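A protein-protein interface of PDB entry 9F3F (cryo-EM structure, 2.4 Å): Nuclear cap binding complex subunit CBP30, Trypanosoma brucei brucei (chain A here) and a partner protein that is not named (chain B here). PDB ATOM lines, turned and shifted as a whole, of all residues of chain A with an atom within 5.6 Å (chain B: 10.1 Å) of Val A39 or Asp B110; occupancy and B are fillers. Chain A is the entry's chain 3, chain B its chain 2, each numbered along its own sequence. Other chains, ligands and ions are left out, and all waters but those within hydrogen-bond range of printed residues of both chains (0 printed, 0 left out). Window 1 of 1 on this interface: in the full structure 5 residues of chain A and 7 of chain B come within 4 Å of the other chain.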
ATOM      1  N   ARG A  35     -37.586  19.681  29.512  1.00  0.00           N
ATOM      2  CA  ARG A  35     -36.351  20.456  29.584  1.00  0.00           C
ATOM      3  C   ARG A  35     -35.266  19.902  28.669  1.00  0.00           C
ATOM      4  O   ARG A  35     -34.390  20.655  28.230  1.00  0.00           O
ATOM      5  CB  ARG A  35     -35.857  20.505  31.028  1.00  0.00           C
ATOM      6  CG  ARG A  35     -35.207  21.815  31.426  1.00  0.00           C
ATOM      7  CD  ARG A  35     -34.891  21.825  32.906  1.00  0.00           C
ATOM      8  NE  ARG A  35     -33.779  22.707  33.229  1.00  0.00           N
ATOM      9  CZ  ARG A  35     -33.231  22.807  34.431  1.00  0.00           C
ATOM     10  NH1 ARG A  35     -33.668  22.089  35.452  1.00  0.00           N
ATOM     11  NH2 ARG A  35     -32.218  23.646  34.616  1.00  0.00           N
ATOM     12  N   GLU A  36     -35.291  18.600  28.374  1.00  0.00           N
ATOM     13  CA  GLU A  36     -34.311  18.045  27.445  1.00  0.00           C
ATOM     14  C   GLU A  36     -34.662  18.378  26.003  1.00  0.00           C
ATOM     15  O   GLU A  36     -33.768  18.523  25.161  1.00  0.00           O
ATOM     16  CB  GLU A  36     -34.204  16.534  27.626  1.00  0.00           C
ATOM     17  CG  GLU A  36     -33.270  16.125  28.731  1.00  0.00           C
ATOM     18  CD  GLU A  36     -33.875  16.343  30.091  1.00  0.00           C
ATOM     19  OE1 GLU A  36     -35.100  16.575  30.174  1.00  0.00           O
ATOM     20  OE2 GLU A  36     -33.127  16.285  31.080  1.00  0.00           O
ATOM     21  N   GLU A  37     -35.954  18.494  25.695  1.00  0.00           N
ATOM     22  CA  GLU A  37     -36.365  18.847  24.343  1.00  0.00           C
ATOM     23  C   GLU A  37     -35.868  20.227  23.936  1.00  0.00           C
ATOM     24  O   GLU A  37     -35.729  20.496  22.738  1.00  0.00           O
ATOM     25  CB  GLU A  37     -37.890  18.781  24.225  1.00  0.00           C
ATOM     26  CG  GLU A  37     -38.411  18.801  22.794  1.00  0.00           C
ATOM     27  CD  GLU A  37     -39.035  20.132  22.418  1.00  0.00           C
ATOM     28  OE1 GLU A  37     -39.715  20.735  23.274  1.00  0.00           O
ATOM     29  OE2 GLU A  37     -38.839  20.577  21.268  1.00  0.00           O
ATOM     30  N   CYS A  38     -35.589  21.102  24.900  1.00  0.00           N
ATOM     31  CA  CYS A  38     -35.111  22.447  24.623  1.00  0.00           C
ATOM     32  C   CYS A  38     -33.598  22.566  24.760  1.00  0.00           C
ATOM     33  O   CYS A  38     -33.080  23.676  24.928  1.00  0.00           O
ATOM     34  CB  CYS A  38     -35.818  23.453  25.533  1.00  0.00           C
ATOM     35  SG  CYS A  38     -35.217  23.513  27.238  1.00  0.00           S
ATOM     36  N   VAL A  39     -32.881  21.452  24.677  1.00  0.00           N
ATOM     37  CA  VAL A  39     -31.429  21.432  24.806  1.00  0.00           C
ATOM     38  C   VAL A  39     -30.824  21.226  23.426  1.00  0.00           C
ATOM     39  O   VAL A  39     -31.093  20.217  22.765  1.00  0.00           O
ATOM     40  CB  VAL A  39     -30.968  20.338  25.780  1.00  0.00           C
ATOM     41  CG1 VAL A  39     -29.487  20.078  25.618  1.00  0.00           C
ATOM     42  CG2 VAL A  39     -31.285  20.738  27.208  1.00  0.00           C
ATOM     43  N   VAL A  40     -30.013  22.186  22.989  1.00  0.00           N
ATOM     44  CA  VAL A  40     -29.280  22.112  21.729  1.00  0.00           C
ATOM     45  C   VAL A  40     -27.818  22.346  22.081  1.00  0.00           C
ATOM     46  O   VAL A  40     -27.457  23.396  22.625  1.00  0.00           O
ATOM     47  CB  VAL A  40     -29.780  23.131  20.702  1.00  0.00           C
ATOM     48  CG1 VAL A  40     -29.156  22.866  19.351  1.00  0.00           C
ATOM     49  CG2 VAL A  40     -31.296  23.097  20.612  1.00  0.00           C
ATOM     50  N   LEU A  41     -26.975  21.371  21.783  1.00  0.00           N
ATOM     51  CA  LEU A  41     -25.615  21.363  22.280  1.00  0.00           C
ATOM     52  C   LEU A  41     -24.725  22.145  21.306  1.00  0.00           C
ATOM     53  O   LEU A  41     -25.062  22.283  20.128  1.00  0.00           O
ATOM     54  CB  LEU A  41     -25.164  19.914  22.434  1.00  0.00           C
ATOM     55  CG  LEU A  41     -24.966  19.287  23.827  1.00  0.00           C
ATOM     56  CD1 LEU A  41     -24.074  18.054  23.766  1.00  0.00           C
ATOM     57  CD2 LEU A  41     -24.520  20.247  24.918  1.00  0.00           C
ATOM     58  N   LEU A  79     -28.355  14.613  22.821  1.00  0.00           N
ATOM     59  CA  LEU A  79     -28.886  15.920  22.476  1.00  0.00           C
ATOM     60  C   LEU A  79     -28.366  16.358  21.109  1.00  0.00           C
ATOM     61  O   LEU A  79     -27.228  16.047  20.748  1.00  0.00           O
ATOM     62  CB  LEU A  79     -28.504  16.947  23.538  1.00  0.00           C
ATOM     63  CG  LEU A  79     -28.871  16.638  24.993  1.00  0.00           C
ATOM     64  CD1 LEU A  79     -30.293  16.093  25.104  1.00  0.00           C
ATOM     65  CD2 LEU A  79     -27.862  15.713  25.664  1.00  0.00           C
ATOM     66  N   PRO A  80     -29.172  17.072  20.330  1.00  0.00           N
ATOM     67  CA  PRO A  80     -28.751  17.468  18.985  1.00  0.00           C
ATOM     68  C   PRO A  80     -27.818  18.664  19.020  1.00  0.00           C
ATOM     69  O   PRO A  80     -28.148  19.706  19.605  1.00  0.00           O
ATOM     70  CB  PRO A  80     -30.076  17.819  18.298  1.00  0.00           C
ATOM     71  CG  PRO A  80     -30.953  18.254  19.401  1.00  0.00           C
ATOM     72  CD  PRO A  80     -30.572  17.434  20.598  1.00  0.00           C
ATOM     73  N   GLY B  47     -26.077  36.426  30.924  1.00  0.00           N
ATOM     74  CA  GLY B  47     -26.584  36.373  29.545  1.00  0.00           C
ATOM     75  C   GLY B  47     -26.775  35.017  28.908  1.00  0.00           C
ATOM     76  O   GLY B  47     -25.860  34.200  28.989  1.00  0.00           O
ATOM     77  N   ASN B  48     -27.907  34.815  28.237  1.00  0.00           N
ATOM     78  CA  ASN B  48     -28.217  33.566  27.489  1.00  0.00           C
ATOM     79  C   ASN B  48     -28.486  32.401  28.440  1.00  0.00           C
ATOM     80  O   ASN B  48     -28.688  31.277  27.942  1.00  0.00           O
ATOM     81  CB  ASN B  48     -27.155  33.217  26.445  1.00  0.00           C
ATOM     82  CG  ASN B  48     -27.651  32.260  25.387  1.00  0.00           C
ATOM     83  OD1 ASN B  48     -28.659  32.518  24.737  1.00  0.00           O
ATOM     84  ND2 ASN B  48     -26.955  31.150  25.213  1.00  0.00           N
ATOM     85  N   LEU B  49     -28.502  32.642  29.746  1.00  0.00           N
ATOM     86  CA  LEU B  49     -28.866  31.552  30.669  1.00  0.00           C
ATOM     87  C   LEU B  49     -30.260  31.099  30.237  1.00  0.00           C
ATOM     88  O   LEU B  49     -30.987  31.906  29.659  1.00  0.00           O
ATOM     89  CB  LEU B  49     -28.820  32.070  32.108  1.00  0.00           C
ATOM     90  CG  LEU B  49     -27.522  32.726  32.551  1.00  0.00           C
ATOM     91  CD1 LEU B  49     -27.692  33.337  33.928  1.00  0.00           C
ATOM     92  CD2 LEU B  49     -26.400  31.709  32.560  1.00  0.00           C
ATOM     93  N   SER B  50     -30.599  29.836  30.468  1.00  0.00           N
ATOM     94  CA  SER B  50     -31.938  29.310  30.116  1.00  0.00           C
ATOM     95  C   SER B  50     -32.977  29.880  31.065  1.00  0.00           C
ATOM     96  O   SER B  50     -32.585  30.459  32.082  1.00  0.00           O
ATOM     97  CB  SER B  50     -31.937  27.822  30.171  1.00  0.00           C
ATOM     98  OG  SER B  50     -32.395  27.364  31.434  1.00  0.00           O
ATOM     99  N   PHE B  51     -34.247  29.673  30.775  1.00  0.00           N
ATOM    100  CA  PHE B  51     -35.241  30.148  31.726  1.00  0.00           C
ATOM    101  C   PHE B  51     -35.339  29.221  32.929  1.00  0.00           C
ATOM    102  O   PHE B  51     -35.744  29.651  34.014  1.00  0.00           O
ATOM    103  CB  PHE B  51     -36.600  30.274  31.044  1.00  0.00           C
ATOM    104  CG  PHE B  51     -36.757  31.518  30.221  1.00  0.00           C
ATOM    105  CD1 PHE B  51     -35.654  32.183  29.722  1.00  0.00           C
ATOM    106  CD2 PHE B  51     -38.014  32.010  29.926  1.00  0.00           C
ATOM    107  CE1 PHE B  51     -35.801  33.318  28.959  1.00  0.00           C
ATOM    108  CE2 PHE B  51     -38.165  33.146  29.162  1.00  0.00           C
ATOM    109  CZ  PHE B  51     -37.057  33.801  28.679  1.00  0.00           C
ATOM    110  N   TYR B  52     -34.970  27.958  32.756  1.00  0.00           N
ATOM    111  CA  TYR B  52     -35.069  26.952  33.799  1.00  0.00           C
ATOM    112  C   TYR B  52     -33.777  26.776  34.575  1.00  0.00           C
ATOM    113  O   TYR B  52     -33.729  25.944  35.487  1.00  0.00           O
ATOM    114  CB  TYR B  52     -35.497  25.615  33.194  1.00  0.00           C
ATOM    115  CG  TYR B  52     -36.733  25.707  32.338  1.00  0.00           C
ATOM    116  CD1 TYR B  52     -37.992  25.558  32.891  1.00  0.00           C
ATOM    117  CD2 TYR B  52     -36.644  25.951  30.978  1.00  0.00           C
ATOM    118  CE1 TYR B  52     -39.126  25.643  32.117  1.00  0.00           C
ATOM    119  CE2 TYR B  52     -37.772  26.040  30.196  1.00  0.00           C
ATOM    120  CZ  TYR B  52     -39.011  25.885  30.770  1.00  0.00           C
ATOM    121  OH  TYR B  52     -40.142  25.972  29.990  1.00  0.00           O
ATOM    122  N   THR B  53     -32.735  27.524  34.243  1.00  0.00           N
ATOM    123  CA  THR B  53     -31.493  27.436  34.990  1.00  0.00           C
ATOM    124  C   THR B  53     -31.701  27.998  36.388  1.00  0.00           C
ATOM    125  O   THR B  53     -32.237  29.097  36.555  1.00  0.00           O
ATOM    126  CB  THR B  53     -30.377  28.188  34.269  1.00  0.00           C
ATOM    127  OG1 THR B  53     -30.187  27.623  32.967  1.00  0.00           O
ATOM    128  CG2 THR B  53     -29.080  28.082  35.040  1.00  0.00           C
ATOM    129  N   GLN B  57     -27.209  26.324  39.866  1.00  0.00           N
ATOM    130  CA  GLN B  57     -26.390  26.052  38.661  1.00  0.00           C
ATOM    131  C   GLN B  57     -25.465  27.252  38.385  1.00  0.00           C
ATOM    132  O   GLN B  57     -24.260  27.015  38.168  1.00  0.00           O
ATOM    133  CB  GLN B  57     -27.329  25.711  37.510  1.00  0.00           C
ATOM    134  CG  GLN B  57     -28.173  24.463  37.720  1.00  0.00           C
ATOM    135  CD  GLN B  57     -28.800  23.980  36.434  1.00  0.00           C
ATOM    136  OE1 GLN B  57     -30.017  24.056  36.240  1.00  0.00           O
ATOM    137  NE2 GLN B  57     -27.962  23.509  35.525  1.00  0.00           N
ATOM    138  N   HIS B  61     -21.218  27.287  39.024  1.00  0.00           N
ATOM    139  CA  HIS B  61     -20.267  27.609  37.935  1.00  0.00           C
ATOM    140  C   HIS B  61     -19.417  28.822  38.308  1.00  0.00           C
ATOM    141  O   HIS B  61     -18.191  28.754  38.130  1.00  0.00           O
ATOM    142  CB  HIS B  61     -21.051  27.833  36.648  1.00  0.00           C
ATOM    143  CG  HIS B  61     -20.254  27.694  35.402  1.00  0.00           C
ATOM    144  ND1 HIS B  61     -20.543  28.423  34.273  1.00  0.00           N
ATOM    145  CD2 HIS B  61     -19.198  26.933  35.098  1.00  0.00           C
ATOM    146  CE1 HIS B  61     -19.685  28.103  33.323  1.00  0.00           C
ATOM    147  NE2 HIS B  61     -18.858  27.200  33.803  1.00  0.00           N
ATOM    148  N   GLY B 105     -18.525  32.430  27.170  1.00  0.00           N
ATOM    149  CA  GLY B 105     -18.628  31.419  26.133  1.00  0.00           C
ATOM    150  C   GLY B 105     -18.413  30.017  26.655  1.00  0.00           C
ATOM    151  O   GLY B 105     -17.843  29.172  25.954  1.00  0.00           O
ATOM    152  N   THR B 106     -18.861  29.751  27.877  1.00  0.00           N
ATOM    153  CA  THR B 106     -18.653  28.475  28.540  1.00  0.00           C
ATOM    154  C   THR B 106     -20.008  27.843  28.824  1.00  0.00           C
ATOM    155  O   THR B 106     -20.948  28.527  29.237  1.00  0.00           O
ATOM    156  CB  THR B 106     -17.853  28.659  29.833  1.00  0.00           C
ATOM    157  OG1 THR B 106     -16.464  28.794  29.515  1.00  0.00           O
ATOM    158  CG2 THR B 106     -18.008  27.471  30.730  1.00  0.00           C
ATOM    159  N   LEU B 107     -20.107  26.540  28.582  1.00  0.00           N
ATOM    160  CA  LEU B 107     -21.370  25.820  28.699  1.00  0.00           C
ATOM    161  C   LEU B 107     -21.778  25.746  30.165  1.00  0.00           C
ATOM    162  O   LEU B 107     -21.071  25.146  30.980  1.00  0.00           O
ATOM    163  CB  LEU B 107     -21.215  24.421  28.114  1.00  0.00           C
ATOM    164  CG  LEU B 107     -22.003  24.085  26.852  1.00  0.00           C
ATOM    165  CD1 LEU B 107     -22.059  22.580  26.638  1.00  0.00           C
ATOM    166  CD2 LEU B 107     -23.374  24.689  26.891  1.00  0.00           C
ATOM    167  N   LEU B 108     -22.914  26.351  30.512  1.00  0.00           N
ATOM    168  CA  LEU B 108     -23.415  26.304  31.881  1.00  0.00           C
ATOM    169  C   LEU B 108     -24.544  25.292  32.043  1.00  0.00           C
ATOM    170  O   LEU B 108     -24.431  24.353  32.835  1.00  0.00           O
ATOM    171  CB  LEU B 108     -23.879  27.696  32.327  1.00  0.00           C
ATOM    172  CG  LEU B 108     -24.593  27.785  33.679  1.00  0.00           C
ATOM    173  CD1 LEU B 108     -23.858  26.999  34.747  1.00  0.00           C
ATOM    174  CD2 LEU B 108     -24.736  29.224  34.108  1.00  0.00           C
ATOM    175  N   ASP B 109     -25.631  25.466  31.303  1.00  0.00           N
ATOM    176  CA  ASP B 109     -26.813  24.619  31.409  1.00  0.00           C
ATOM    177  C   ASP B 109     -27.266  24.189  30.028  1.00  0.00           C
ATOM    178  O   ASP B 109     -28.429  24.343  29.649  1.00  0.00           O
ATOM    179  CB  ASP B 109     -27.938  25.335  32.146  1.00  0.00           C
ATOM    180  CG  ASP B 109     -29.033  24.390  32.593  1.00  0.00           C
ATOM    181  OD1 ASP B 109     -28.718  23.234  32.940  1.00  0.00           O
ATOM    182  OD2 ASP B 109     -30.211  24.802  32.595  1.00  0.00           O
ATOM    183  N   ASP B 110     -26.325  23.662  29.245  1.00  0.00           N
ATOM    184  CA  ASP B 110     -26.531  23.391  27.825  1.00  0.00           C
ATOM    185  C   ASP B 110     -26.837  24.674  27.062  1.00  0.00           C
ATOM    186  O   ASP B 110     -27.542  24.661  26.052  1.00  0.00           O
ATOM    187  CB  ASP B 110     -27.627  22.346  27.599  1.00  0.00           C
ATOM    188  CG  ASP B 110     -27.574  21.217  28.610  1.00  0.00           C
ATOM    189  OD1 ASP B 110     -26.516  20.561  28.715  1.00  0.00           O
ATOM    190  OD2 ASP B 110     -28.590  20.986  29.298  1.00  0.00           O
ATOM    191  N   ARG B 111     -26.309  25.790  27.558  1.00  0.00           N
ATOM    192  CA  ARG B 111     -26.415  27.089  26.914  1.00  0.00           C
ATOM    193  C   ARG B 111     -25.076  27.796  27.043  1.00  0.00           C
ATOM    194  O   ARG B 111     -24.507  27.845  28.135  1.00  0.00           O
ATOM    195  CB  ARG B 111     -27.519  27.931  27.547  1.00  0.00           C
ATOM    196  CG  ARG B 111     -28.909  27.525  27.152  1.00  0.00           C
ATOM    197  CD  ARG B 111     -29.413  28.347  25.996  1.00  0.00           C
ATOM    198  NE  ARG B 111     -30.830  28.647  26.137  1.00  0.00           N
ATOM    199  CZ  ARG B 111     -31.357  29.855  26.009  1.00  0.00           C
ATOM    200  NH1 ARG B 111     -30.609  30.908  25.727  1.00  0.00           N
ATOM    201  NH2 ARG B 111     -32.668  30.012  26.168  1.00  0.00           N
ATOM    202  N   VAL B 112     -24.574  28.332  25.938  1.00  0.00           N
ATOM    203  CA  VAL B 112     -23.314  29.065  25.956  1.00  0.00           C
ATOM    204  C   VAL B 112     -23.590  30.476  26.458  1.00  0.00           C
ATOM    205  O   VAL B 112     -24.406  31.201  25.882  1.00  0.00           O
ATOM    206  CB  VAL B 112     -22.664  29.083  24.566  1.00  0.00           C
ATOM    207  CG1 VAL B 112     -21.193  29.398  24.680  1.00  0.00           C
ATOM    208  CG2 VAL B 112     -22.870  27.750  23.871  1.00  0.00           C
ATOM    209  N   ILE B 113     -22.911  30.866  27.531  1.00  0.00           N
ATOM    210  CA  ILE B 113     -23.224  32.103  28.230  1.00  0.00           C
ATOM    211  C   ILE B 113     -22.296  33.213  27.751  1.00  0.00           C
ATOM    212  O   ILE B 113     -21.263  32.971  27.123  1.00  0.00           O
ATOM    213  CB  ILE B 113     -23.140  31.918  29.757  1.00  0.00           C
ATOM    214  CG1 ILE B 113     -21.698  31.694  30.194  1.00  0.00           C
ATOM    215  CG2 ILE B 113     -24.010  30.758  30.192  1.00  0.00           C
ATOM    216  CD1 ILE B 113     -21.563  31.219  31.613  1.00  0.00           C
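The guanidinium group (NH2) of Arg A35 lies within hydrogen-bond range of the backbone carbonyl oxygen (O) of Tyr B52 (2.9 Å).
OE1 of Gln B57 lies within hydrogen-bond range of NH2 of Arg A35 (2.8 Å).
OD2 of Asp B109 is in salt-bridge range of NH2 of Arg A35.
The backbone NH (N) of Tyr B52 sits at hydrogen-bond distance from the side-chain hydroxyl (OG) of Ser B50.
The side-chain hydroxyl of Thr B53 is in hydrogen-bond range of the side-chain hydroxyl of Ser B50 (2.7 Å).
OG1 of Thr B53 is in hydrogen-bond range of OD2 of Asp B109, 2.8 Å away.
OD1 of Asp B109 lies within hydrogen-bond range of NE2 of Gln B57 (2.7 Å).
O of Arg A35 lies within hydrogen-bond range of SG of Cys A38 (3.1 Å).
N of Leu A41 is in hydrogen-bond range of O of Pro A80 (3.0 Å).
Arg A35 touches Thr B53 (NH2 to CA, 3.9 Å).
Val A39 touches Asp B110.
O of Val A40 touches O of Asp B110, 3.7 Å away.
Leu B107 touches Leu A41.
Glu A37 touches none of the printed residues of chain B.
Cys A38 touches none of the printed residues of chain B.
Val A39 touches just one residue of chain B: Asp B110.
Val A40 touches just one residue of chain B: Asp B110 (3.7 Å).
Printed residues of chain A within 4 Å of Tyr B52: Arg A35 (2.9 Å).
Gly B105 touches none of the printed residues of chain A.
Of the printed residues of chain A, Asp B109 touches Arg A35.
Asp B110 touches two residues of chain A.
The nearest residue of chain B that does not touch Val A39 is Asp B109 (5.2 Å).
The nearest residue of chain A that does not touch Asp B110 is Leu A41 (4.3 Å).
The nearest printed residue of chain B that does not touch Leu A41 is Asp B110 (4.3 Å).
Of the 18 printed residues of chain B, 6 touch a printed residue of chain A.
Hydrophobic or aromatic side chains of chain B that line the printed part of chain A: Tyr B52 and Leu B107.
Hydrophobic or aromatic side chains of chain A within 4 Å of the printed part of chain B: Val A39 and Leu A41.
Along chain A the printed residues that touch a printed residue of chain B span positions 35 to 41.
Among the printed residues, 7 pairs touch across the chains.
Among the printed residues, Asp or Glu carboxylates within 4 Å of a Lys or Arg side-chain nitrogen of the other chain: Arg A35 with Asp B109 (3.1 Å).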
